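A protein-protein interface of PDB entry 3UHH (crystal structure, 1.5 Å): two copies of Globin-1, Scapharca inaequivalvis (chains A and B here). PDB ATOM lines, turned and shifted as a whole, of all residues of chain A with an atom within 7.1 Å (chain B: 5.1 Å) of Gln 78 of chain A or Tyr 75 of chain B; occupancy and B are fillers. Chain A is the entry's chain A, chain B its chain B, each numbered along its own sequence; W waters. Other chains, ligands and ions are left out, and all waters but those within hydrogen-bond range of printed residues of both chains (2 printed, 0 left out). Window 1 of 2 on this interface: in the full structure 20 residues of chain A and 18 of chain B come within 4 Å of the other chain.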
ATOM      1  N   TRP A  22      -2.393  -5.881  -1.892  1.00  0.00           N
ATOM      2  CA  TRP A  22      -3.243  -5.743  -3.069  1.00  0.00           C
ATOM      3  C   TRP A  22      -4.567  -5.077  -2.728  1.00  0.00           C
ATOM      4  O   TRP A  22      -5.137  -4.365  -3.551  1.00  0.00           O
ATOM      5  CB  TRP A  22      -3.515  -7.105  -3.714  1.00  0.00           C
ATOM      6  CG  TRP A  22      -4.365  -6.994  -4.951  1.00  0.00           C
ATOM      7  CD1 TRP A  22      -5.645  -7.449  -5.115  1.00  0.00           C
ATOM      8  CD2 TRP A  22      -4.005  -6.351  -6.182  1.00  0.00           C
ATOM      9  NE1 TRP A  22      -6.102  -7.126  -6.371  1.00  0.00           N
ATOM     10  CE2 TRP A  22      -5.118  -6.455  -7.045  1.00  0.00           C
ATOM     11  CE3 TRP A  22      -2.851  -5.700  -6.636  1.00  0.00           C
ATOM     12  CZ2 TRP A  22      -5.108  -5.925  -8.343  1.00  0.00           C
ATOM     13  CZ3 TRP A  22      -2.843  -5.174  -7.925  1.00  0.00           C
ATOM     14  CH2 TRP A  22      -3.967  -5.293  -8.763  1.00  0.00           C
ATOM     15  N   GLY A  26      -4.721  -2.356  -5.386  1.00  0.00           N
ATOM     16  CA  GLY A  26      -5.724  -2.781  -6.349  1.00  0.00           C
ATOM     17  C   GLY A  26      -7.028  -2.000  -6.298  1.00  0.00           C
ATOM     18  O   GLY A  26      -7.892  -2.181  -7.159  1.00  0.00           O
ATOM     19  N   SER A  27      -7.177  -1.133  -5.299  1.00  0.00           N
ATOM     20  CA  SER A  27      -8.396  -0.336  -5.144  1.00  0.00           C
ATOM     21  C   SER A  27      -8.494   0.801  -6.158  1.00  0.00           C
ATOM     22  O   SER A  27      -9.580   1.322  -6.417  1.00  0.00           O
ATOM     23  CB  SER A  27      -8.482   0.239  -3.727  1.00  0.00           C
ATOM     24  OG  SER A  27      -7.447   1.177  -3.491  1.00  0.00           O
ATOM     25  N   LYS A  29      -7.095   0.897  -9.703  1.00  0.00           N
ATOM     26  CA  LYS A  29      -6.406   0.306 -10.838  1.00  0.00           C
ATOM     27  C   LYS A  29      -5.947   1.312 -11.886  1.00  0.00           C
ATOM     28  O   LYS A  29      -4.859   1.177 -12.438  1.00  0.00           O
ATOM     29  CB  LYS A  29      -7.293  -0.767 -11.473  1.00  0.00           C
ATOM     30  CG  LYS A  29      -7.536  -1.952 -10.551  1.00  0.00           C
ATOM     31  CD  LYS A  29      -8.324  -3.051 -11.242  1.00  0.00           C
ATOM     32  CE  LYS A  29      -8.455  -4.279 -10.355  1.00  0.00           C
ATOM     33  NZ  LYS A  29      -9.176  -3.984  -9.087  1.00  0.00           N
ATOM     34  N   THR A  72      -5.722  -2.511 -17.834  1.00  0.00           N
ATOM     35  CA  THR A  72      -5.733  -3.932 -18.155  1.00  0.00           C
ATOM     36  C   THR A  72      -4.597  -4.680 -17.459  1.00  0.00           C
ATOM     37  O   THR A  72      -4.762  -5.823 -17.038  1.00  0.00           O
ATOM     38  CB  THR A  72      -5.654  -4.141 -19.680  1.00  0.00           C
ATOM     39  OG1 THR A  72      -6.768  -3.483 -20.299  1.00  0.00           O
ATOM     40  CG2 THR A  72      -5.695  -5.624 -20.023  1.00  0.00           C
ATOM     41  N   LEU A  73      -3.444  -4.031 -17.327  1.00  0.00           N
ATOM     42  CA  LEU A  73      -2.309  -4.655 -16.655  1.00  0.00           C
ATOM     43  C   LEU A  73      -2.691  -4.983 -15.209  1.00  0.00           C
ATOM     44  O   LEU A  73      -2.328  -6.038 -14.681  1.00  0.00           O
ATOM     45  CB  LEU A  73      -1.092  -3.717 -16.690  1.00  0.00           C
ATOM     46  CG  LEU A  73       0.193  -4.168 -15.983  1.00  0.00           C
ATOM     47  CD1 LEU A  73       1.393  -3.470 -16.604  1.00  0.00           C
ATOM     48  CD2 LEU A  73       0.101  -3.866 -14.493  1.00  0.00           C
ATOM     49  N   MET A  74      -3.433  -4.081 -14.572  1.00  0.00           N
ATOM     50  CA  MET A  74      -3.847  -4.294 -13.193  1.00  0.00           C
ATOM     51  C   MET A  74      -4.804  -5.471 -13.055  1.00  0.00           C
ATOM     52  O   MET A  74      -4.849  -6.119 -12.012  1.00  0.00           O
ATOM     53  CB  MET A  74      -4.476  -3.024 -12.618  1.00  0.00           C
ATOM     54  CG  MET A  74      -3.490  -1.867 -12.469  1.00  0.00           C
ATOM     55  SD  MET A  74      -2.123  -2.225 -11.331  1.00  0.00           S
ATOM     56  CE  MET A  74      -2.833  -1.689  -9.799  1.00  0.00           C
ATOM     57  N   TYR A  75      -5.570  -5.754 -14.104  1.00  0.00           N
ATOM     58  CA  TYR A  75      -6.488  -6.885 -14.049  1.00  0.00           C
ATOM     59  C   TYR A  75      -5.742  -8.199 -14.221  1.00  0.00           C
ATOM     60  O   TYR A  75      -6.252  -9.262 -13.870  1.00  0.00           O
ATOM     61  CB  TYR A  75      -7.597  -6.730 -15.091  1.00  0.00           C
ATOM     62  CG  TYR A  75      -8.705  -5.833 -14.591  1.00  0.00           C
ATOM     63  CD1 TYR A  75      -9.672  -6.319 -13.710  1.00  0.00           C
ATOM     64  CD2 TYR A  75      -8.745  -4.488 -14.935  1.00  0.00           C
ATOM     65  CE1 TYR A  75     -10.656  -5.477 -13.185  1.00  0.00           C
ATOM     66  CE2 TYR A  75      -9.717  -3.640 -14.415  1.00  0.00           C
ATOM     67  CZ  TYR A  75     -10.667  -4.139 -13.540  1.00  0.00           C
ATOM     68  OH  TYR A  75     -11.619  -3.294 -13.019  1.00  0.00           O
ATOM     69  N   ALA A  76      -4.526  -8.130 -14.758  1.00  0.00           N
ATOM     70  CA  ALA A  76      -3.709  -9.330 -14.897  1.00  0.00           C
ATOM     71  C   ALA A  76      -3.229  -9.663 -13.483  1.00  0.00           C
ATOM     72  O   ALA A  76      -3.209 -10.824 -13.075  1.00  0.00           O
ATOM     73  CB  ALA A  76      -2.520  -9.066 -15.812  1.00  0.00           C
ATOM     74  N   LEU A  77      -2.850  -8.632 -12.730  1.00  0.00           N
ATOM     75  CA  LEU A  77      -2.398  -8.835 -11.359  1.00  0.00           C
ATOM     76  C   LEU A  77      -3.562  -9.325 -10.497  1.00  0.00           C
ATOM     77  O   LEU A  77      -3.377 -10.180  -9.635  1.00  0.00           O
ATOM     78  CB  LEU A  77      -1.810  -7.538 -10.784  1.00  0.00           C
ATOM     79  CG  LEU A  77      -0.522  -7.047 -11.454  1.00  0.00           C
ATOM     80  CD1 LEU A  77      -0.039  -5.787 -10.754  1.00  0.00           C
ATOM     81  CD2 LEU A  77       0.545  -8.134 -11.399  1.00  0.00           C
ATOM     82  N   GLN A  78      -4.759  -8.789 -10.738  1.00  0.00           N
ATOM     83  CA  GLN A  78      -5.946  -9.205  -9.992  1.00  0.00           C
ATOM     84  C   GLN A  78      -6.154 -10.700 -10.229  1.00  0.00           C
ATOM     85  O   GLN A  78      -6.472 -11.456  -9.310  1.00  0.00           O
ATOM     86  CB  GLN A  78      -7.173  -8.432 -10.481  1.00  0.00           C
ATOM     87  CG  GLN A  78      -8.481  -8.845  -9.810  1.00  0.00           C
ATOM     88  CD  GLN A  78      -8.553  -8.420  -8.361  1.00  0.00           C
ATOM     89  OE1 GLN A  78      -8.423  -7.240  -8.044  1.00  0.00           O
ATOM     90  NE2 GLN A  78      -8.770  -9.382  -7.469  1.00  0.00           N
ATOM     91  N   ASN A  79      -5.965 -11.108 -11.479  1.00  0.00           N
ATOM     92  CA  ASN A  79      -6.101 -12.498 -11.898  1.00  0.00           C
ATOM     93  C   ASN A  79      -5.150 -13.371 -11.069  1.00  0.00           C
ATOM     94  O   ASN A  79      -5.568 -14.353 -10.456  1.00  0.00           O
ATOM     95  CB  ASN A  79      -5.756 -12.591 -13.389  1.00  0.00           C
ATOM     96  CG  ASN A  79      -6.160 -13.907 -14.021  1.00  0.00           C
ATOM     97  OD1 ASN A  79      -6.287 -14.930 -13.349  1.00  0.00           O
ATOM     98  ND2 ASN A  79      -6.341 -13.888 -15.338  1.00  0.00           N
ATOM     99  N   PHE A  80      -3.871 -13.003 -11.045  1.00  0.00           N
ATOM    100  CA  PHE A  80      -2.873 -13.758 -10.285  1.00  0.00           C
ATOM    101  C   PHE A  80      -3.262 -13.894  -8.816  1.00  0.00           C
ATOM    102  O   PHE A  80      -3.197 -14.983  -8.245  1.00  0.00           O
ATOM    103  CB  PHE A  80      -1.499 -13.080 -10.354  1.00  0.00           C
ATOM    104  CG  PHE A  80      -0.905 -13.009 -11.736  1.00  0.00           C
ATOM    105  CD1 PHE A  80      -1.307 -13.881 -12.742  1.00  0.00           C
ATOM    106  CD2 PHE A  80       0.096 -12.083 -12.015  1.00  0.00           C
ATOM    107  CE1 PHE A  80      -0.718 -13.832 -14.007  1.00  0.00           C
ATOM    108  CE2 PHE A  80       0.692 -12.024 -13.273  1.00  0.00           C
ATOM    109  CZ  PHE A  80       0.285 -12.900 -14.271  1.00  0.00           C
ATOM    110  N   ILE A  81      -3.655 -12.785  -8.201  1.00  0.00           N
ATOM    111  CA  ILE A  81      -4.034 -12.804  -6.795  1.00  0.00           C
ATOM    112  C   ILE A  81      -5.199 -13.757  -6.551  1.00  0.00           C
ATOM    113  O   ILE A  81      -5.200 -14.506  -5.574  1.00  0.00           O
ATOM    114  CB  ILE A  81      -4.419 -11.389  -6.306  1.00  0.00           C
ATOM    115  CG1 ILE A  81      -3.196 -10.468  -6.368  1.00  0.00           C
ATOM    116  CG2 ILE A  81      -4.985 -11.454  -4.891  1.00  0.00           C
ATOM    117  CD1 ILE A  81      -2.033 -10.905  -5.490  1.00  0.00           C
ATOM    118  N   ASP A  82      -6.185 -13.737  -7.442  1.00  0.00           N
ATOM    119  CA  ASP A  82      -7.344 -14.613  -7.288  1.00  0.00           C
ATOM    120  C   ASP A  82      -7.016 -16.096  -7.469  1.00  0.00           C
ATOM    121  O   ASP A  82      -7.774 -16.956  -7.017  1.00  0.00           O
ATOM    122  CB  ASP A  82      -8.457 -14.222  -8.270  1.00  0.00           C
ATOM    123  CG  ASP A  82      -9.144 -12.916  -7.898  1.00  0.00           C
ATOM    124  OD1 ASP A  82      -9.080 -12.511  -6.718  1.00  0.00           O
ATOM    125  OD2 ASP A  82      -9.771 -12.298  -8.785  1.00  0.00           O
ATOM    126  N   GLN A  83      -5.894 -16.402  -8.118  1.00  0.00           N
ATOM    127  CA  GLN A  83      -5.510 -17.795  -8.345  1.00  0.00           C
ATOM    128  C   GLN A  83      -4.524 -18.343  -7.315  1.00  0.00           C
ATOM    129  O   GLN A  83      -4.068 -19.477  -7.441  1.00  0.00           O
ATOM    130  CB  GLN A  83      -4.884 -17.972  -9.734  1.00  0.00           C
ATOM    131  CG  GLN A  83      -5.638 -17.336 -10.888  1.00  0.00           C
ATOM    132  CD  GLN A  83      -7.131 -17.584 -10.838  1.00  0.00           C
ATOM    133  OE1 GLN A  83      -7.581 -18.692 -10.551  1.00  0.00           O
ATOM    134  NE2 GLN A  83      -7.907 -16.548 -11.132  1.00  0.00           N
ATOM    135  N   VAL A  93      -2.585 -19.382 -15.976  1.00  0.00           N
ATOM    136  CA  VAL A  93      -2.836 -17.985 -16.321  1.00  0.00           C
ATOM    137  C   VAL A  93      -1.503 -17.260 -16.487  1.00  0.00           C
ATOM    138  O   VAL A  93      -1.379 -16.359 -17.313  1.00  0.00           O
ATOM    139  CB  VAL A  93      -3.688 -17.259 -15.251  1.00  0.00           C
ATOM    140  CG1 VAL A  93      -5.106 -17.814 -15.250  1.00  0.00           C
ATOM    141  CG2 VAL A  93      -3.055 -17.408 -13.883  1.00  0.00           C
ATOM    142  N   PHE A  97      -0.061 -15.183 -19.954  1.00  0.00           N
ATOM    143  CA  PHE A  97       0.522 -13.852 -20.042  1.00  0.00           C
ATOM    144  C   PHE A  97       1.984 -13.897 -20.458  1.00  0.00           C
ATOM    145  O   PHE A  97       2.498 -12.948 -21.056  1.00  0.00           O
ATOM    146  CB  PHE A  97       0.354 -13.113 -18.714  1.00  0.00           C
ATOM    147  CG  PHE A  97      -1.051 -12.640 -18.476  1.00  0.00           C
ATOM    148  CD1 PHE A  97      -1.633 -11.713 -19.337  1.00  0.00           C
ATOM    149  CD2 PHE A  97      -1.807 -13.143 -17.426  1.00  0.00           C
ATOM    150  CE1 PHE A  97      -2.951 -11.296 -19.157  1.00  0.00           C
ATOM    151  CE2 PHE A  97      -3.128 -12.732 -17.237  1.00  0.00           C
ATOM    152  CZ  PHE A  97      -3.700 -11.808 -18.105  1.00  0.00           C
ATOM    153  N   TRP A 135       6.102  -9.418  -3.615  1.00  0.00           N
ATOM    154  CA  TRP A 135       5.719  -9.216  -5.005  1.00  0.00           C
ATOM    155  C   TRP A 135       6.791  -9.693  -5.977  1.00  0.00           C
ATOM    156  O   TRP A 135       6.481 -10.114  -7.090  1.00  0.00           O
ATOM    157  CB  TRP A 135       5.388  -7.745  -5.267  1.00  0.00           C
ATOM    158  CG  TRP A 135       4.002  -7.392  -4.840  1.00  0.00           C
ATOM    159  CD1 TRP A 135       3.606  -6.953  -3.609  1.00  0.00           C
ATOM    160  CD2 TRP A 135       2.812  -7.545  -5.613  1.00  0.00           C
ATOM    161  NE1 TRP A 135       2.239  -6.826  -3.569  1.00  0.00           N
ATOM    162  CE2 TRP A 135       1.724  -7.180  -4.793  1.00  0.00           C
ATOM    163  CE3 TRP A 135       2.555  -7.953  -6.932  1.00  0.00           C
ATOM    164  CZ2 TRP A 135       0.399  -7.219  -5.234  1.00  0.00           C
ATOM    165  CZ3 TRP A 135       1.236  -7.992  -7.375  1.00  0.00           C
ATOM    166  CH2 TRP A 135       0.175  -7.622  -6.527  1.00  0.00           C
ATOM    167  N   LYS B  29     -15.313 -17.635 -12.319  1.00  0.00           N
ATOM    168  CA  LYS B  29     -14.663 -17.338 -13.584  1.00  0.00           C
ATOM    169  C   LYS B  29     -14.118 -18.555 -14.316  1.00  0.00           C
ATOM    170  O   LYS B  29     -14.216 -18.634 -15.537  1.00  0.00           O
ATOM    171  CB  LYS B  29     -13.568 -16.292 -13.364  1.00  0.00           C
ATOM    172  CG  LYS B  29     -14.133 -14.952 -12.909  1.00  0.00           C
ATOM    173  CD  LYS B  29     -13.058 -13.890 -12.790  1.00  0.00           C
ATOM    174  CE  LYS B  29     -13.659 -12.503 -12.610  1.00  0.00           C
ATOM    175  NZ  LYS B  29     -14.480 -12.386 -11.376  1.00  0.00           N
ATOM    176  N   ILE B  71     -10.196 -18.198 -18.210  1.00  0.00           N
ATOM    177  CA  ILE B  71     -10.198 -17.421 -16.979  1.00  0.00           C
ATOM    178  C   ILE B  71      -9.879 -15.966 -17.322  1.00  0.00           C
ATOM    179  O   ILE B  71     -10.533 -15.044 -16.838  1.00  0.00           O
ATOM    180  CB  ILE B  71      -9.150 -17.951 -15.975  1.00  0.00           C
ATOM    181  CG1 ILE B  71      -9.586 -19.321 -15.447  1.00  0.00           C
ATOM    182  CG2 ILE B  71      -8.972 -16.960 -14.823  1.00  0.00           C
ATOM    183  CD1 ILE B  71      -8.523 -20.015 -14.620  1.00  0.00           C
ATOM    184  N   THR B  72      -8.876 -15.767 -18.173  1.00  0.00           N
ATOM    185  CA  THR B  72      -8.472 -14.425 -18.570  1.00  0.00           C
ATOM    186  C   THR B  72      -9.586 -13.694 -19.324  1.00  0.00           C
ATOM    187  O   THR B  72      -9.760 -12.482 -19.172  1.00  0.00           O
ATOM    188  CB  THR B  72      -7.186 -14.485 -19.419  1.00  0.00           C
ATOM    189  OG1 THR B  72      -6.157 -15.127 -18.654  1.00  0.00           O
ATOM    190  CG2 THR B  72      -6.720 -13.088 -19.796  1.00  0.00           C
ATOM    191  N   LEU B  73     -10.353 -14.427 -20.123  1.00  0.00           N
ATOM    192  CA  LEU B  73     -11.450 -13.814 -20.859  1.00  0.00           C
ATOM    193  C   LEU B  73     -12.450 -13.207 -19.869  1.00  0.00           C
ATOM    194  O   LEU B  73     -12.988 -12.121 -20.097  1.00  0.00           O
ATOM    195  CB  LEU B  73     -12.141 -14.859 -21.747  1.00  0.00           C
ATOM    196  CG  LEU B  73     -13.361 -14.419 -22.565  1.00  0.00           C
ATOM    197  CD1 LEU B  73     -13.503 -15.313 -23.789  1.00  0.00           C
ATOM    198  CD2 LEU B  73     -14.616 -14.472 -21.706  1.00  0.00           C
ATOM    199  N   MET B  74     -12.688 -13.905 -18.761  1.00  0.00           N
ATOM    200  CA  MET B  74     -13.626 -13.424 -17.753  1.00  0.00           C
ATOM    201  C   MET B  74     -13.140 -12.159 -17.057  1.00  0.00           C
ATOM    202  O   MET B  74     -13.946 -11.380 -16.553  1.00  0.00           O
ATOM    203  CB  MET B  74     -13.912 -14.522 -16.721  1.00  0.00           C
ATOM    204  CG  MET B  74     -14.634 -15.744 -17.295  1.00  0.00           C
ATOM    205  SD  MET B  74     -16.275 -15.373 -17.969  1.00  0.00           S
ATOM    206  CE  MET B  74     -17.290 -15.613 -16.524  1.00  0.00           C
ATOM    207  N   TYR B  75     -11.824 -11.952 -17.018  1.00  0.00           N
ATOM    208  CA  TYR B  75     -11.297 -10.740 -16.399  1.00  0.00           C
ATOM    209  C   TYR B  75     -11.417  -9.552 -17.349  1.00  0.00           C
ATOM    210  O   TYR B  75     -11.386  -8.403 -16.916  1.00  0.00           O
ATOM    211  CB  TYR B  75      -9.852 -10.949 -15.946  1.00  0.00           C
ATOM    212  CG  TYR B  75      -9.779 -11.648 -14.610  1.00  0.00           C
ATOM    213  CD1 TYR B  75      -9.957 -10.940 -13.420  1.00  0.00           C
ATOM    214  CD2 TYR B  75      -9.606 -13.028 -14.535  1.00  0.00           C
ATOM    215  CE1 TYR B  75      -9.963 -11.593 -12.190  1.00  0.00           C
ATOM    216  CE2 TYR B  75      -9.615 -13.688 -13.315  1.00  0.00           C
ATOM    217  CZ  TYR B  75      -9.797 -12.967 -12.148  1.00  0.00           C
ATOM    218  OH  TYR B  75      -9.838 -13.627 -10.945  1.00  0.00           O
ATOM    219  N   ALA B  76     -11.559  -9.827 -18.643  1.00  0.00           N
ATOM    220  CA  ALA B  76     -11.755  -8.762 -19.621  1.00  0.00           C
ATOM    221  C   ALA B  76     -13.177  -8.268 -19.368  1.00  0.00           C
ATOM    222  O   ALA B  76     -13.443  -7.068 -19.381  1.00  0.00           O
ATOM    223  CB  ALA B  76     -11.628  -9.304 -21.044  1.00  0.00           C
ATOM    224  N   LEU B  77     -14.091  -9.203 -19.127  1.00  0.00           N
ATOM    225  CA  LEU B  77     -15.469  -8.830 -18.844  1.00  0.00           C
ATOM    226  C   LEU B  77     -15.550  -8.113 -17.495  1.00  0.00           C
ATOM    227  O   LEU B  77     -16.318  -7.163 -17.338  1.00  0.00           O
ATOM    228  CB  LEU B  77     -16.373 -10.066 -18.851  1.00  0.00           C
ATOM    229  CG  LEU B  77     -16.514 -10.771 -20.205  1.00  0.00           C
ATOM    230  CD1 LEU B  77     -17.483 -11.942 -20.067  1.00  0.00           C
ATOM    231  CD2 LEU B  77     -17.025  -9.791 -21.259  1.00  0.00           C
ATOM    232  N   GLN B  78     -14.762  -8.562 -16.520  1.00  0.00           N
ATOM    233  CA  GLN B  78     -14.751  -7.917 -15.209  1.00  0.00           C
ATOM    234  C   GLN B  78     -14.337  -6.461 -15.403  1.00  0.00           C
ATOM    235  O   GLN B  78     -14.914  -5.549 -14.812  1.00  0.00           O
ATOM    236  CB  GLN B  78     -13.747  -8.604 -14.281  1.00  0.00           C
ATOM    237  CG  GLN B  78     -13.663  -7.988 -12.890  1.00  0.00           C
ATOM    238  CD  GLN B  78     -14.902  -8.254 -12.069  1.00  0.00           C
ATOM    239  OE1 GLN B  78     -15.282  -9.406 -11.864  1.00  0.00           O
ATOM    240  NE2 GLN B  78     -15.539  -7.192 -11.587  1.00  0.00           N
ATOM    241  N   ASN B  79     -13.323  -6.271 -16.239  1.00  0.00           N
ATOM    242  CA  ASN B  79     -12.789  -4.954 -16.565  1.00  0.00           C
ATOM    243  C   ASN B  79     -13.925  -4.079 -17.113  1.00  0.00           C
ATOM    244  O   ASN B  79     -14.167  -2.975 -16.624  1.00  0.00           O
ATOM    245  CB  ASN B  79     -11.685  -5.122 -17.615  1.00  0.00           C
ATOM    246  CG  ASN B  79     -10.820  -3.890 -17.779  1.00  0.00           C
ATOM    247  OD1 ASN B  79     -11.216  -2.782 -17.431  1.00  0.00           O
ATOM    248  ND2 ASN B  79      -9.629  -4.083 -18.341  1.00  0.00           N
HETATM  249  O   HOH W   1     -12.574 -14.120  -9.044  1.00  0.00           O
HETATM  250  O   HOH W   2     -11.022 -16.229 -10.344  1.00  0.00           O
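The side-chain carboxylate (OD2) of Asp 82 of chain A lies within hydrogen-bond range of the side-chain hydroxyl (OH) of Tyr 75 of chain B.
OE1 of Gln 78 of chain B sits at hydrogen-bond distance from NZ of Lys 29 of chain B, at 3.1 Å.
The side-chain carboxylate (OD1) of Asp 82 of chain A sits at hydrogen-bond distance from the side-chain amide nitrogen (NE2) of Gln 78 of chain A, at 3.2 Å.
The side-chain amide oxygen of Asn 79 of chain A is in hydrogen-bond range of the side-chain amide nitrogen of Gln 83 of chain A.
NE1 of Trp 22 of chain A is in hydrogen-bond range of OE1 of Gln 78 of chain A, 2.9 Å away.
Asn 79 of chain B touches Thr 72 of chain A (ND2 to OG1, 3.5 Å).
Gln 78 of chain B touches Tyr 75 of chain A.
Tyr 75 of chain A touches Asn 79 of chain B.
Asn 79 of chain A touches Ile 71 of chain B.
Asn 79 of chain A touches Thr 72 of chain B (ND2 to OG1, 3.5 Å).
Asn 79 of chain A touches Tyr 75 of chain B.
Gln 83 of chain A touches Ile 71 of chain B (NE2 to CG2, 3.9 Å).
NE2 of Gln 83 of chain A touches OH of Tyr 75 of chain B, 3.5 Å away.
CG1 of Val 93 of chain A touches CG2 of Ile 71 of chain B, at 3.98 Å.
Thr 72 of chain B touches Phe 97 of chain A.
Ser 27 of chain A touches none of the printed residues of chain B.
Printed residues of chain B within 4 Å of Thr 72 of chain A: Asn 79 (3.5 Å).
Of chain B, only Tyr 75 comes within 4 Å of Gln 78 of chain A.
Printed residues of chain B within 4 Å of Asn 79 of chain A: Ile 71 (3.7 Å), Thr 72 (3.5 Å) and Tyr 75 (3.5 Å).
Phe 80 of chain A touches none of the printed residues of chain B.
Of the printed residues of chain B, Phe 97 of chain A touches Thr 72.
Of chain A, only Gln 78 (3.9 Å), Asn 79 (3.5 Å), Asp 82 (2.5 Å) and Gln 83 (3.5 Å) come within 4 Å of Tyr 75 of chain B.
Of the printed residues of chain A, Asn 79 of chain B touches Thr 72 and Tyr 75.
The nearest residue of chain A that does not touch Tyr 75 of chain B is Tyr 75 of chain A (4.1 Å).
Hydrophobic or aromatic side chains of chain B within 4 Å of the printed part of chain A: Ile 71 and Tyr 75.
Along chain B the printed residues that touch a printed residue of chain A span positions 71 to 79.
Printed residues of chain A that touch a printed residue of chain B: Thr 72, Tyr 75, Gln 78, Asn 79, Asp 82, Gln 83, Val 93 and Phe 97.
Hydrophobic or aromatic side chains of chain A within 4 Å of the printed part of chain B: Tyr 75, Val 93 and Phe 97.
Thr 72 of chain A touches Asn 79 of chain B, and with the chains exchanged Asn 79 of chain A touches Thr 72 of chain B.
Tyr 75 of chain A touches Gln 78 of chain B, and with the chains exchanged Gln 78 of chain A touches Tyr 75 of chain B.
Tyr 75 of chain A touches Asn 79 of chain B, and with the chains exchanged Asn 79 of chain A touches Tyr 75 of chain B.
Positions printed for both chains: 29, 72, 73, 74, 75, 76, 77, 78 and 79.
Water W2 bridges the side-chain hydroxyl (OH) of Tyr 75 of chain B and the side-chain amide nitrogen (NE2) of Gln 83 of chain A.
Water W1 lies within hydrogen-bond range of the side-chain carboxylate (OD2) of Asp 82 of chain A (3.4 Å), the side-chain hydroxyl (OH) of Tyr 75 of chain B (3.4 Å) and the side-chain amino group (NZ) of Lys 29 of chain B (3.5 Å).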
